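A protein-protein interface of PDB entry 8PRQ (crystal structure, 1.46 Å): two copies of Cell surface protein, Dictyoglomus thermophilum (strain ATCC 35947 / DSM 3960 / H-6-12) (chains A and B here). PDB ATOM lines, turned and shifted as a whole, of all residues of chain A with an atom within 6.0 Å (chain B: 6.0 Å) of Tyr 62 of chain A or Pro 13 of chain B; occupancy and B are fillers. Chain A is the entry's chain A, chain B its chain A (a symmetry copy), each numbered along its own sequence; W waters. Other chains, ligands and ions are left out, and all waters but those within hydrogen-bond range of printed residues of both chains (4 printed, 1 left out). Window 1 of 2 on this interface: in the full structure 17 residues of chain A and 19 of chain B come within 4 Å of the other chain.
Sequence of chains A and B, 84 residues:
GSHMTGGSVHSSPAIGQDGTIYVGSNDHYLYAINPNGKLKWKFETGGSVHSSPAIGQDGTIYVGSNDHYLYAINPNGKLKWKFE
The side-chain hydroxyl of Ser 51 of chain A sits at hydrogen-bond distance from the backbone carbonyl oxygen of Ser 11 of chain B (2.7 Å).
N of Ser 52 of chain A sits at hydrogen-bond distance from OG of Ser 12 of chain B (2.8 Å).
The backbone carbonyl oxygen (O) of Pro 35 of chain B is in hydrogen-bond range of the indole nitrogen (NE1) of Trp 81 of chain A, 2.9 Å away.
2 positions are printed for both chains.
Of the 16 pairs that touch across the chains among the printed residues, none has its exchanged pair printed and touching as well.
Among the printed residues, pairs that only touch across the chains: Ser 51 of chain A with Val 9 of chain B, Ser 51 of chain A with Ser 12 of chain B, Ser 51 of chain A with Pro 13 of chain B, Ser 52 of chain A with Pro 13 of chain B, Ala 54 of chain A with Pro 13 of chain B, Ala 54 of chain A with Ile 15 of chain B, Ile 55 of chain A with Ile 15 of chain B, Gly 56 of chain A with Ile 15 of chain B, Tyr 62 of chain A with Pro 13 of chain B, Tyr 62 of chain A with Ile 15 of chain B, Tyr 62 of chain A with Ile 21 of chain B, Gly 64 of chain A with Val 9 of chain B and Leu 70 of chain A with Ile 21 of chain B.
Water W4 bridges the side-chain hydroxyl of Tyr 62 of chain A and the backbone carbonyl oxygen of Pro 35 of chain B.
Water W3 bridges the backbone carbonyl oxygen of Val 9 of chain B and the backbone NH of Ser 51 of chain A.
Water W1 lies within hydrogen-bond range of the side-chain hydroxyl of Ser 52 of chain A and the side-chain hydroxyl of Ser 12 of chain B.
Water W2 lies within hydrogen-bond range of the backbone carbonyl oxygen (O) of Gly 19 of chain B (2.8 Å) and the side-chain hydroxyl (OH) of Tyr 62 of chain A (2.8 Å).
Printed residues of chain A that touch a printed residue of chain B: Ser 51, Ser 52, Ala 54, Ile 55, Gly 56, Tyr 62, Gly 64, Leu 70 and Trp 81.
Hydrophobic or aromatic side chains of chain A that line the printed part of chain B: Ala 54, Tyr 62, Leu 70 and Trp 81.
Of the 13 printed residues of chain B, 7 touch a printed residue of chain A.
Among the printed residues, 16 pairs touch across the chains.
Of chain B, only Pro 13, Ile 15 and Ile 21 come within 4 Å of Tyr 62 of chain A.
Of the printed residues of chain B, Gly 64 of chain A touches Val 9 (3.6 Å).
Printed residues of chain A within 4 Å of Ser 12 of chain B: Ser 51 (3.6 Å) and Ser 52 (2.8 Å).
Asp 58 of chain A touches none of the printed residues of chain B.
Gly 19 of chain B touches none of the printed residues of chain A.
The nearest residue of chain B that does not touch Tyr 62 of chain A is Pro 35 of chain B (4.7 Å).
The nearest printed residue of chain A that does not touch Pro 13 of chain B is Val 63 of chain A (4.3 Å).
N of Gly 64 of chain A sits at hydrogen-bond distance from OG of Ser 51 of chain A (3.0 Å).
N of Tyr 62 of chain A is in hydrogen-bond range of O of Ala 54 of chain A.
The backbone NH (N) of Ala 72 of chain A sits at hydrogen-bond distance from the backbone carbonyl oxygen (O) of Trp 81 of chain A.
The backbone NH (N) of Ser 12 of chain B sits at hydrogen-bond distance from the side-chain hydroxyl (OG) of Ser 52 of chain B (2.9 Å).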
ATOM      1  N   SER A  51     -18.455  11.300   8.404  1.00  0.00           N
ATOM      2  CA  SER A  51     -18.348  11.879   7.061  1.00  0.00           C
ATOM      3  C   SER A  51     -17.428  13.096   7.059  1.00  0.00           C
ATOM      4  O   SER A  51     -17.315  13.821   8.044  1.00  0.00           O
ATOM      5  CB  SER A  51     -19.768  12.274   6.649  1.00  0.00           C
ATOM      6  OG  SER A  51     -19.876  12.778   5.320  1.00  0.00           O
ATOM      7  N   SER A  52     -16.760  13.328   5.898  1.00  0.00           N
ATOM      8  CA  SER A  52     -15.852  14.463   5.750  1.00  0.00           C
ATOM      9  C   SER A  52     -16.545  15.561   4.971  1.00  0.00           C
ATOM     10  O   SER A  52     -17.145  15.280   3.918  1.00  0.00           O
ATOM     11  CB  SER A  52     -14.574  14.040   5.030  1.00  0.00           C
ATOM     12  OG  SER A  52     -13.924  12.978   5.738  1.00  0.00           O
ATOM     13  N   PRO A  53     -16.486  16.808   5.429  1.00  0.00           N
ATOM     14  CA  PRO A  53     -17.272  17.868   4.776  1.00  0.00           C
ATOM     15  C   PRO A  53     -16.737  18.244   3.408  1.00  0.00           C
ATOM     16  O   PRO A  53     -15.541  18.141   3.121  1.00  0.00           O
ATOM     17  CB  PRO A  53     -17.173  19.047   5.749  1.00  0.00           C
ATOM     18  CG  PRO A  53     -16.029  18.737   6.660  1.00  0.00           C
ATOM     19  CD  PRO A  53     -15.861  17.258   6.693  1.00  0.00           C
ATOM     20  N   ALA A  54     -17.667  18.688   2.573  1.00  0.00           N
ATOM     21  CA  ALA A  54     -17.383  19.283   1.279  1.00  0.00           C
ATOM     22  C   ALA A  54     -17.936  20.703   1.266  1.00  0.00           C
ATOM     23  O   ALA A  54     -18.913  21.014   1.950  1.00  0.00           O
ATOM     24  CB  ALA A  54     -18.027  18.469   0.148  1.00  0.00           C
ATOM     25  N   ILE A  55     -17.317  21.570   0.461  1.00  0.00           N
ATOM     26  CA  ILE A  55     -17.684  22.979   0.419  1.00  0.00           C
ATOM     27  C   ILE A  55     -18.156  23.289  -0.986  1.00  0.00           C
ATOM     28  O   ILE A  55     -17.421  23.064  -1.962  1.00  0.00           O
ATOM     29  CB  ILE A  55     -16.525  23.894   0.819  1.00  0.00           C
ATOM     30  CG1 ILE A  55     -16.002  23.539   2.209  1.00  0.00           C
ATOM     31  CG2 ILE A  55     -16.994  25.335   0.833  1.00  0.00           C
ATOM     32  CD1 ILE A  55     -14.751  24.292   2.638  1.00  0.00           C
ATOM     33  N   GLY A  56     -19.364  23.825  -1.094  1.00  0.00           N
ATOM     34  CA  GLY A  56     -19.911  24.206  -2.379  1.00  0.00           C
ATOM     35  C   GLY A  56     -19.413  25.566  -2.852  1.00  0.00           C
ATOM     36  O   GLY A  56     -18.716  26.298  -2.151  1.00  0.00           O
ATOM     37  N   ASP A  58     -20.849  28.345  -3.263  1.00  0.00           N
ATOM     38  CA  ASP A  58     -21.323  29.480  -2.477  1.00  0.00           C
ATOM     39  C   ASP A  58     -20.903  29.402  -1.022  1.00  0.00           C
ATOM     40  O   ASP A  58     -21.356  30.212  -0.208  1.00  0.00           O
ATOM     41  CB  ASP A  58     -22.843  29.614  -2.574  1.00  0.00           C
ATOM     42  CG  ASP A  58     -23.592  28.439  -1.965  1.00  0.00           C
ATOM     43  OD1 ASP A  58     -22.946  27.468  -1.504  1.00  0.00           O
ATOM     44  OD2 ASP A  58     -24.850  28.496  -1.961  1.00  0.00           O
ATOM     45  N   THR A  60     -21.438  26.885   1.116  1.00  0.00           N
ATOM     46  CA  THR A  60     -22.226  25.971   1.941  1.00  0.00           C
ATOM     47  C   THR A  60     -21.366  24.764   2.268  1.00  0.00           C
ATOM     48  O   THR A  60     -20.622  24.268   1.418  1.00  0.00           O
ATOM     49  CB  THR A  60     -23.461  25.497   1.175  1.00  0.00           C
ATOM     50  OG1 THR A  60     -24.258  26.624   0.778  1.00  0.00           O
ATOM     51  CG2 THR A  60     -24.339  24.592   2.034  1.00  0.00           C
ATOM     52  N   ILE A  61     -21.492  24.275   3.501  1.00  0.00           N
ATOM     53  CA  ILE A  61     -20.754  23.101   3.963  1.00  0.00           C
ATOM     54  C   ILE A  61     -21.725  21.934   4.044  1.00  0.00           C
ATOM     55  O   ILE A  61     -22.787  22.051   4.654  1.00  0.00           O
ATOM     56  CB  ILE A  61     -20.057  23.369   5.307  1.00  0.00           C
ATOM     57  CG1 ILE A  61     -19.212  24.656   5.224  1.00  0.00           C
ATOM     58  CG2 ILE A  61     -19.183  22.180   5.725  1.00  0.00           C
ATOM     59  CD1 ILE A  61     -19.864  25.838   5.856  1.00  0.00           C
ATOM     60  N   TYR A  62     -21.378  20.835   3.391  1.00  0.00           N
ATOM     61  CA  TYR A  62     -22.191  19.623   3.398  1.00  0.00           C
ATOM     62  C   TYR A  62     -21.437  18.515   4.106  1.00  0.00           C
ATOM     63  O   TYR A  62     -20.254  18.304   3.848  1.00  0.00           O
ATOM     64  CB  TYR A  62     -22.467  19.146   1.985  1.00  0.00           C
ATOM     65  CG  TYR A  62     -23.035  20.208   1.079  1.00  0.00           C
ATOM     66  CD1 TYR A  62     -24.397  20.437   1.037  1.00  0.00           C
ATOM     67  CD2 TYR A  62     -22.218  20.961   0.265  1.00  0.00           C
ATOM     68  CE1 TYR A  62     -24.947  21.382   0.204  1.00  0.00           C
ATOM     69  CE2 TYR A  62     -22.751  21.941  -0.579  1.00  0.00           C
ATOM     70  CZ  TYR A  62     -24.118  22.151  -0.597  1.00  0.00           C
ATOM     71  OH  TYR A  62     -24.626  23.114  -1.452  1.00  0.00           O
ATOM     72  N   VAL A  63     -22.142  17.776   4.967  1.00  0.00           N
ATOM     73  CA  VAL A  63     -21.525  16.666   5.679  1.00  0.00           C
ATOM     74  C   VAL A  63     -22.619  15.697   6.093  1.00  0.00           C
ATOM     75  O   VAL A  63     -23.737  16.092   6.431  1.00  0.00           O
ATOM     76  CB  VAL A  63     -20.707  17.190   6.884  1.00  0.00           C
ATOM     77  CG1 VAL A  63     -21.628  17.587   8.017  1.00  0.00           C
ATOM     78  CG2 VAL A  63     -19.644  16.176   7.312  1.00  0.00           C
ATOM     79  N   GLY A  64     -22.294  14.431   6.051  1.00  0.00           N
ATOM     80  CA  GLY A  64     -23.201  13.435   6.596  1.00  0.00           C
ATOM     81  C   GLY A  64     -23.030  13.199   8.081  1.00  0.00           C
ATOM     82  O   GLY A  64     -22.048  13.585   8.718  1.00  0.00           O
ATOM     83  N   LEU A  70     -27.899  14.006   5.584  1.00  0.00           N
ATOM     84  CA  LEU A  70     -26.899  14.862   4.962  1.00  0.00           C
ATOM     85  C   LEU A  70     -27.291  16.274   5.348  1.00  0.00           C
ATOM     86  O   LEU A  70     -28.436  16.673   5.126  1.00  0.00           O
ATOM     87  CB  LEU A  70     -26.935  14.726   3.445  1.00  0.00           C
ATOM     88  CG  LEU A  70     -26.007  15.679   2.718  1.00  0.00           C
ATOM     89  CD1 LEU A  70     -24.559  15.300   2.887  1.00  0.00           C
ATOM     90  CD2 LEU A  70     -26.394  15.694   1.257  1.00  0.00           C
ATOM     91  N   TYR A  71     -26.351  17.013   5.938  1.00  0.00           N
ATOM     92  CA  TYR A  71     -26.561  18.379   6.382  1.00  0.00           C
ATOM     93  C   TYR A  71     -25.937  19.367   5.424  1.00  0.00           C
ATOM     94  O   TYR A  71     -24.836  19.142   4.922  1.00  0.00           O
ATOM     95  CB  TYR A  71     -25.897  18.578   7.744  1.00  0.00           C
ATOM     96  CG  TYR A  71     -26.686  17.963   8.843  1.00  0.00           C
ATOM     97  CD1 TYR A  71     -26.491  16.640   9.185  1.00  0.00           C
ATOM     98  CD2 TYR A  71     -27.615  18.697   9.539  1.00  0.00           C
ATOM     99  CE1 TYR A  71     -27.215  16.050  10.208  1.00  0.00           C
ATOM    100  CE2 TYR A  71     -28.356  18.128  10.552  1.00  0.00           C
ATOM    101  CZ  TYR A  71     -28.150  16.805  10.889  1.00  0.00           C
ATOM    102  OH  TYR A  71     -28.883  16.248  11.914  1.00  0.00           O
ATOM    103  N   ALA A  72     -26.641  20.472   5.217  1.00  0.00           N
ATOM    104  CA  ALA A  72     -26.131  21.627   4.483  1.00  0.00           C
ATOM    105  C   ALA A  72     -26.113  22.794   5.465  1.00  0.00           C
ATOM    106  O   ALA A  72     -27.169  23.250   5.901  1.00  0.00           O
ATOM    107  CB  ALA A  72     -27.044  21.964   3.297  1.00  0.00           C
ATOM    108  N   ILE A  73     -24.920  23.262   5.812  1.00  0.00           N
ATOM    109  CA  ILE A  73     -24.742  24.325   6.789  1.00  0.00           C
ATOM    110  C   ILE A  73     -24.286  25.570   6.042  1.00  0.00           C
ATOM    111  O   ILE A  73     -23.488  25.475   5.104  1.00  0.00           O
ATOM    112  CB  ILE A  73     -23.702  23.906   7.842  1.00  0.00           C
ATOM    113  CG1 ILE A  73     -23.983  22.476   8.351  1.00  0.00           C
ATOM    114  CG2 ILE A  73     -23.635  24.881   9.002  1.00  0.00           C
ATOM    115  CD1 ILE A  73     -25.385  22.295   8.897  1.00  0.00           C
ATOM    116  N   LYS A  80     -28.886  25.254   6.731  1.00  0.00           N
ATOM    117  CA  LYS A  80     -29.548  25.557   5.465  1.00  0.00           C
ATOM    118  C   LYS A  80     -30.655  24.538   5.189  1.00  0.00           C
ATOM    119  O   LYS A  80     -31.815  24.917   5.013  1.00  0.00           O
ATOM    120  CB  LYS A  80     -28.524  25.560   4.325  1.00  0.00           C
ATOM    121  CG  LYS A  80     -29.054  26.033   2.962  1.00  0.00           C
ATOM    122  CD  LYS A  80     -27.885  26.368   2.028  1.00  0.00           C
ATOM    123  CE  LYS A  80     -28.311  26.939   0.699  1.00  0.00           C
ATOM    124  NZ  LYS A  80     -29.491  27.841   0.781  1.00  0.00           N
ATOM    125  N   TRP A  81     -30.309  23.247   5.118  1.00  0.00           N
ATOM    126  CA  TRP A  81     -31.304  22.178   5.116  1.00  0.00           C
ATOM    127  C   TRP A  81     -30.644  20.892   5.599  1.00  0.00           C
ATOM    128  O   TRP A  81     -29.425  20.804   5.727  1.00  0.00           O
ATOM    129  CB  TRP A  81     -31.962  21.969   3.743  1.00  0.00           C
ATOM    130  CG  TRP A  81     -31.044  21.962   2.551  1.00  0.00           C
ATOM    131  CD1 TRP A  81     -30.886  22.974   1.647  1.00  0.00           C
ATOM    132  CD2 TRP A  81     -30.190  20.902   2.112  1.00  0.00           C
ATOM    133  NE1 TRP A  81     -29.977  22.613   0.677  1.00  0.00           N
ATOM    134  CE2 TRP A  81     -29.536  21.341   0.945  1.00  0.00           C
ATOM    135  CE3 TRP A  81     -29.906  19.621   2.597  1.00  0.00           C
ATOM    136  CZ2 TRP A  81     -28.623  20.547   0.254  1.00  0.00           C
ATOM    137  CZ3 TRP A  81     -28.991  18.827   1.905  1.00  0.00           C
ATOM    138  CH2 TRP A  81     -28.358  19.298   0.748  1.00  0.00           C
ATOM    139  N   VAL B   9     -24.825   8.145   7.217  1.00  0.00           N
ATOM    140  CA  VAL B   9     -24.107   8.690   6.070  1.00  0.00           C
ATOM    141  C   VAL B   9     -22.643   8.729   6.490  1.00  0.00           C
ATOM    142  O   VAL B   9     -22.169   9.719   7.045  1.00  0.00           O
ATOM    143  CB  VAL B   9     -24.639  10.068   5.665  1.00  0.00           C
ATOM    144  CG1 VAL B   9     -23.865  10.578   4.451  1.00  0.00           C
ATOM    145  CG2 VAL B   9     -26.137   9.998   5.366  1.00  0.00           C
ATOM    146  N   SER B  11     -20.270   8.018   4.138  1.00  0.00           N
ATOM    147  CA  SER B  11     -19.680   8.541   2.908  1.00  0.00           C
ATOM    148  C   SER B  11     -19.525  10.051   2.993  1.00  0.00           C
ATOM    149  O   SER B  11     -20.300  10.741   3.660  1.00  0.00           O
ATOM    150  CB  SER B  11     -20.657   8.183   1.800  1.00  0.00           C
ATOM    151  OG  SER B  11     -20.160   8.464   0.515  1.00  0.00           O
ATOM    152  N   SER B  12     -18.512  10.573   2.272  1.00  0.00           N
ATOM    153  CA  SER B  12     -18.230  12.003   2.268  1.00  0.00           C
ATOM    154  C   SER B  12     -18.714  12.599   0.959  1.00  0.00           C
ATOM    155  O   SER B  12     -18.428  12.045  -0.111  1.00  0.00           O
ATOM    156  CB  SER B  12     -16.728  12.255   2.431  1.00  0.00           C
ATOM    157  OG  SER B  12     -16.275  11.684   3.665  1.00  0.00           O
ATOM    158  N   PRO B  13     -19.446  13.703   0.995  1.00  0.00           N
ATOM    159  CA  PRO B  13     -20.072  14.212  -0.233  1.00  0.00           C
ATOM    160  C   PRO B  13     -19.086  14.751  -1.250  1.00  0.00           C
ATOM    161  O   PRO B  13     -18.002  15.253  -0.925  1.00  0.00           O
ATOM    162  CB  PRO B  13     -21.004  15.321   0.273  1.00  0.00           C
ATOM    163  CG  PRO B  13     -20.491  15.683   1.635  1.00  0.00           C
ATOM    164  CD  PRO B  13     -19.936  14.405   2.206  1.00  0.00           C
ATOM    165  N   ALA B  14     -19.498  14.633  -2.508  1.00  0.00           N
ATOM    166  CA  ALA B  14     -18.844  15.265  -3.645  1.00  0.00           C
ATOM    167  C   ALA B  14     -19.823  16.228  -4.296  1.00  0.00           C
ATOM    168  O   ALA B  14     -21.035  16.027  -4.274  1.00  0.00           O
ATOM    169  CB  ALA B  14     -18.394  14.199  -4.643  1.00  0.00           C
ATOM    170  N   ILE B  15     -19.290  17.294  -4.891  1.00  0.00           N
ATOM    171  CA  ILE B  15     -20.119  18.358  -5.447  1.00  0.00           C
ATOM    172  C   ILE B  15     -19.828  18.452  -6.927  1.00  0.00           C
ATOM    173  O   ILE B  15     -18.666  18.601  -7.328  1.00  0.00           O
ATOM    174  CB  ILE B  15     -19.877  19.694  -4.729  1.00  0.00           C
ATOM    175  CG1 ILE B  15     -20.083  19.527  -3.214  1.00  0.00           C
ATOM    176  CG2 ILE B  15     -20.797  20.768  -5.277  1.00  0.00           C
ATOM    177  CD1 ILE B  15     -19.583  20.684  -2.407  1.00  0.00           C
ATOM    178  N   GLY B  19     -23.593  21.997  -8.817  1.00  0.00           N
ATOM    179  CA  GLY B  19     -23.870  22.098  -7.409  1.00  0.00           C
ATOM    180  C   GLY B  19     -24.538  20.879  -6.847  1.00  0.00           C
ATOM    181  O   GLY B  19     -24.784  20.825  -5.629  1.00  0.00           O
ATOM    182  N   ILE B  21     -25.096  17.508  -5.048  1.00  0.00           N
ATOM    183  CA  ILE B  21     -24.329  16.887  -3.978  1.00  0.00           C
ATOM    184  C   ILE B  21     -24.571  15.393  -4.068  1.00  0.00           C
ATOM    185  O   ILE B  21     -25.723  14.958  -4.071  1.00  0.00           O
ATOM    186  CB  ILE B  21     -24.720  17.439  -2.596  1.00  0.00           C
ATOM    187  CG1 ILE B  21     -24.657  18.976  -2.604  1.00  0.00           C
ATOM    188  CG2 ILE B  21     -23.804  16.879  -1.528  1.00  0.00           C
ATOM    189  CD1 ILE B  21     -26.004  19.639  -2.781  1.00  0.00           C
ATOM    190  N   TYR B  22     -23.489  14.619  -4.162  1.00  0.00           N
ATOM    191  CA  TYR B  22     -23.545  13.164  -4.230  1.00  0.00           C
ATOM    192  C   TYR B  22     -22.957  12.582  -2.952  1.00  0.00           C
ATOM    193  O   TYR B  22     -21.869  12.976  -2.525  1.00  0.00           O
ATOM    194  CB  TYR B  22     -22.730  12.650  -5.416  1.00  0.00           C
ATOM    195  CG  TYR B  22     -23.102  13.260  -6.738  1.00  0.00           C
ATOM    196  CD1 TYR B  22     -24.166  12.763  -7.483  1.00  0.00           C
ATOM    197  CD2 TYR B  22     -22.392  14.327  -7.250  1.00  0.00           C
ATOM    198  CE1 TYR B  22     -24.516  13.327  -8.700  1.00  0.00           C
ATOM    199  CE2 TYR B  22     -22.727  14.887  -8.468  1.00  0.00           C
ATOM    200  CZ  TYR B  22     -23.783  14.373  -9.184  1.00  0.00           C
ATOM    201  OH  TYR B  22     -24.108  14.932 -10.398  1.00  0.00           O
ATOM    202  N   VAL B  23     -23.641  11.588  -2.383  1.00  0.00           N
ATOM    203  CA  VAL B  23     -23.167  10.966  -1.147  1.00  0.00           C
ATOM    204  C   VAL B  23     -23.767   9.577  -1.029  1.00  0.00           C
ATOM    205  O   VAL B  23     -24.913   9.334  -1.407  1.00  0.00           O
ATOM    206  CB  VAL B  23     -23.484  11.846   0.087  1.00  0.00           C
ATOM    207  CG1 VAL B  23     -24.926  11.729   0.499  1.00  0.00           C
ATOM    208  CG2 VAL B  23     -22.561  11.523   1.240  1.00  0.00           C
ATOM    209  N   PRO B  35     -29.036  21.356  -4.930  1.00  0.00           N
ATOM    210  CA  PRO B  35     -28.554  22.331  -3.945  1.00  0.00           C
ATOM    211  C   PRO B  35     -29.648  22.907  -3.054  1.00  0.00           C
ATOM    212  O   PRO B  35     -29.335  23.456  -1.987  1.00  0.00           O
ATOM    213  CB  PRO B  35     -27.857  23.397  -4.803  1.00  0.00           C
ATOM    214  CG  PRO B  35     -28.220  23.082  -6.204  1.00  0.00           C
ATOM    215  CD  PRO B  35     -28.573  21.654  -6.295  1.00  0.00           C
ATOM    216  N   SER B  52     -16.545   7.252  -0.693  1.00  0.00           N
ATOM    217  CA  SER B  52     -16.938   8.620  -1.022  1.00  0.00           C
ATOM    218  C   SER B  52     -16.844   8.823  -2.520  1.00  0.00           C
ATOM    219  O   SER B  52     -15.822   8.453  -3.125  1.00  0.00           O
ATOM    220  CB  SER B  52     -16.042   9.626  -0.304  1.00  0.00           C
ATOM    221  OG  SER B  52     -16.094   9.425   1.114  1.00  0.00           O
ATOM    222  N   PRO B  53     -17.860   9.402  -3.154  1.00  0.00           N
ATOM    223  CA  PRO B  53     -17.860   9.477  -4.624  1.00  0.00           C
ATOM    224  C   PRO B  53     -16.838  10.455  -5.167  1.00  0.00           C
ATOM    225  O   PRO B  53     -16.480  11.450  -4.532  1.00  0.00           O
ATOM    226  CB  PRO B  53     -19.286   9.923  -4.965  1.00  0.00           C
ATOM    227  CG  PRO B  53     -19.864  10.465  -3.697  1.00  0.00           C
ATOM    228  CD  PRO B  53     -19.148   9.826  -2.560  1.00  0.00           C
HETATM  229  O   HOH W   1     -14.895  10.490   6.403  1.00  0.00           O
HETATM  230  O   HOH W   2     -23.700  22.850  -4.066  1.00  0.00           O
HETATM  231  O   HOH W   3     -21.219  10.144   9.526  1.00  0.00           O
HETATM  232  O   HOH W   4     -26.870  24.213  -0.935  1.00  0.00           O
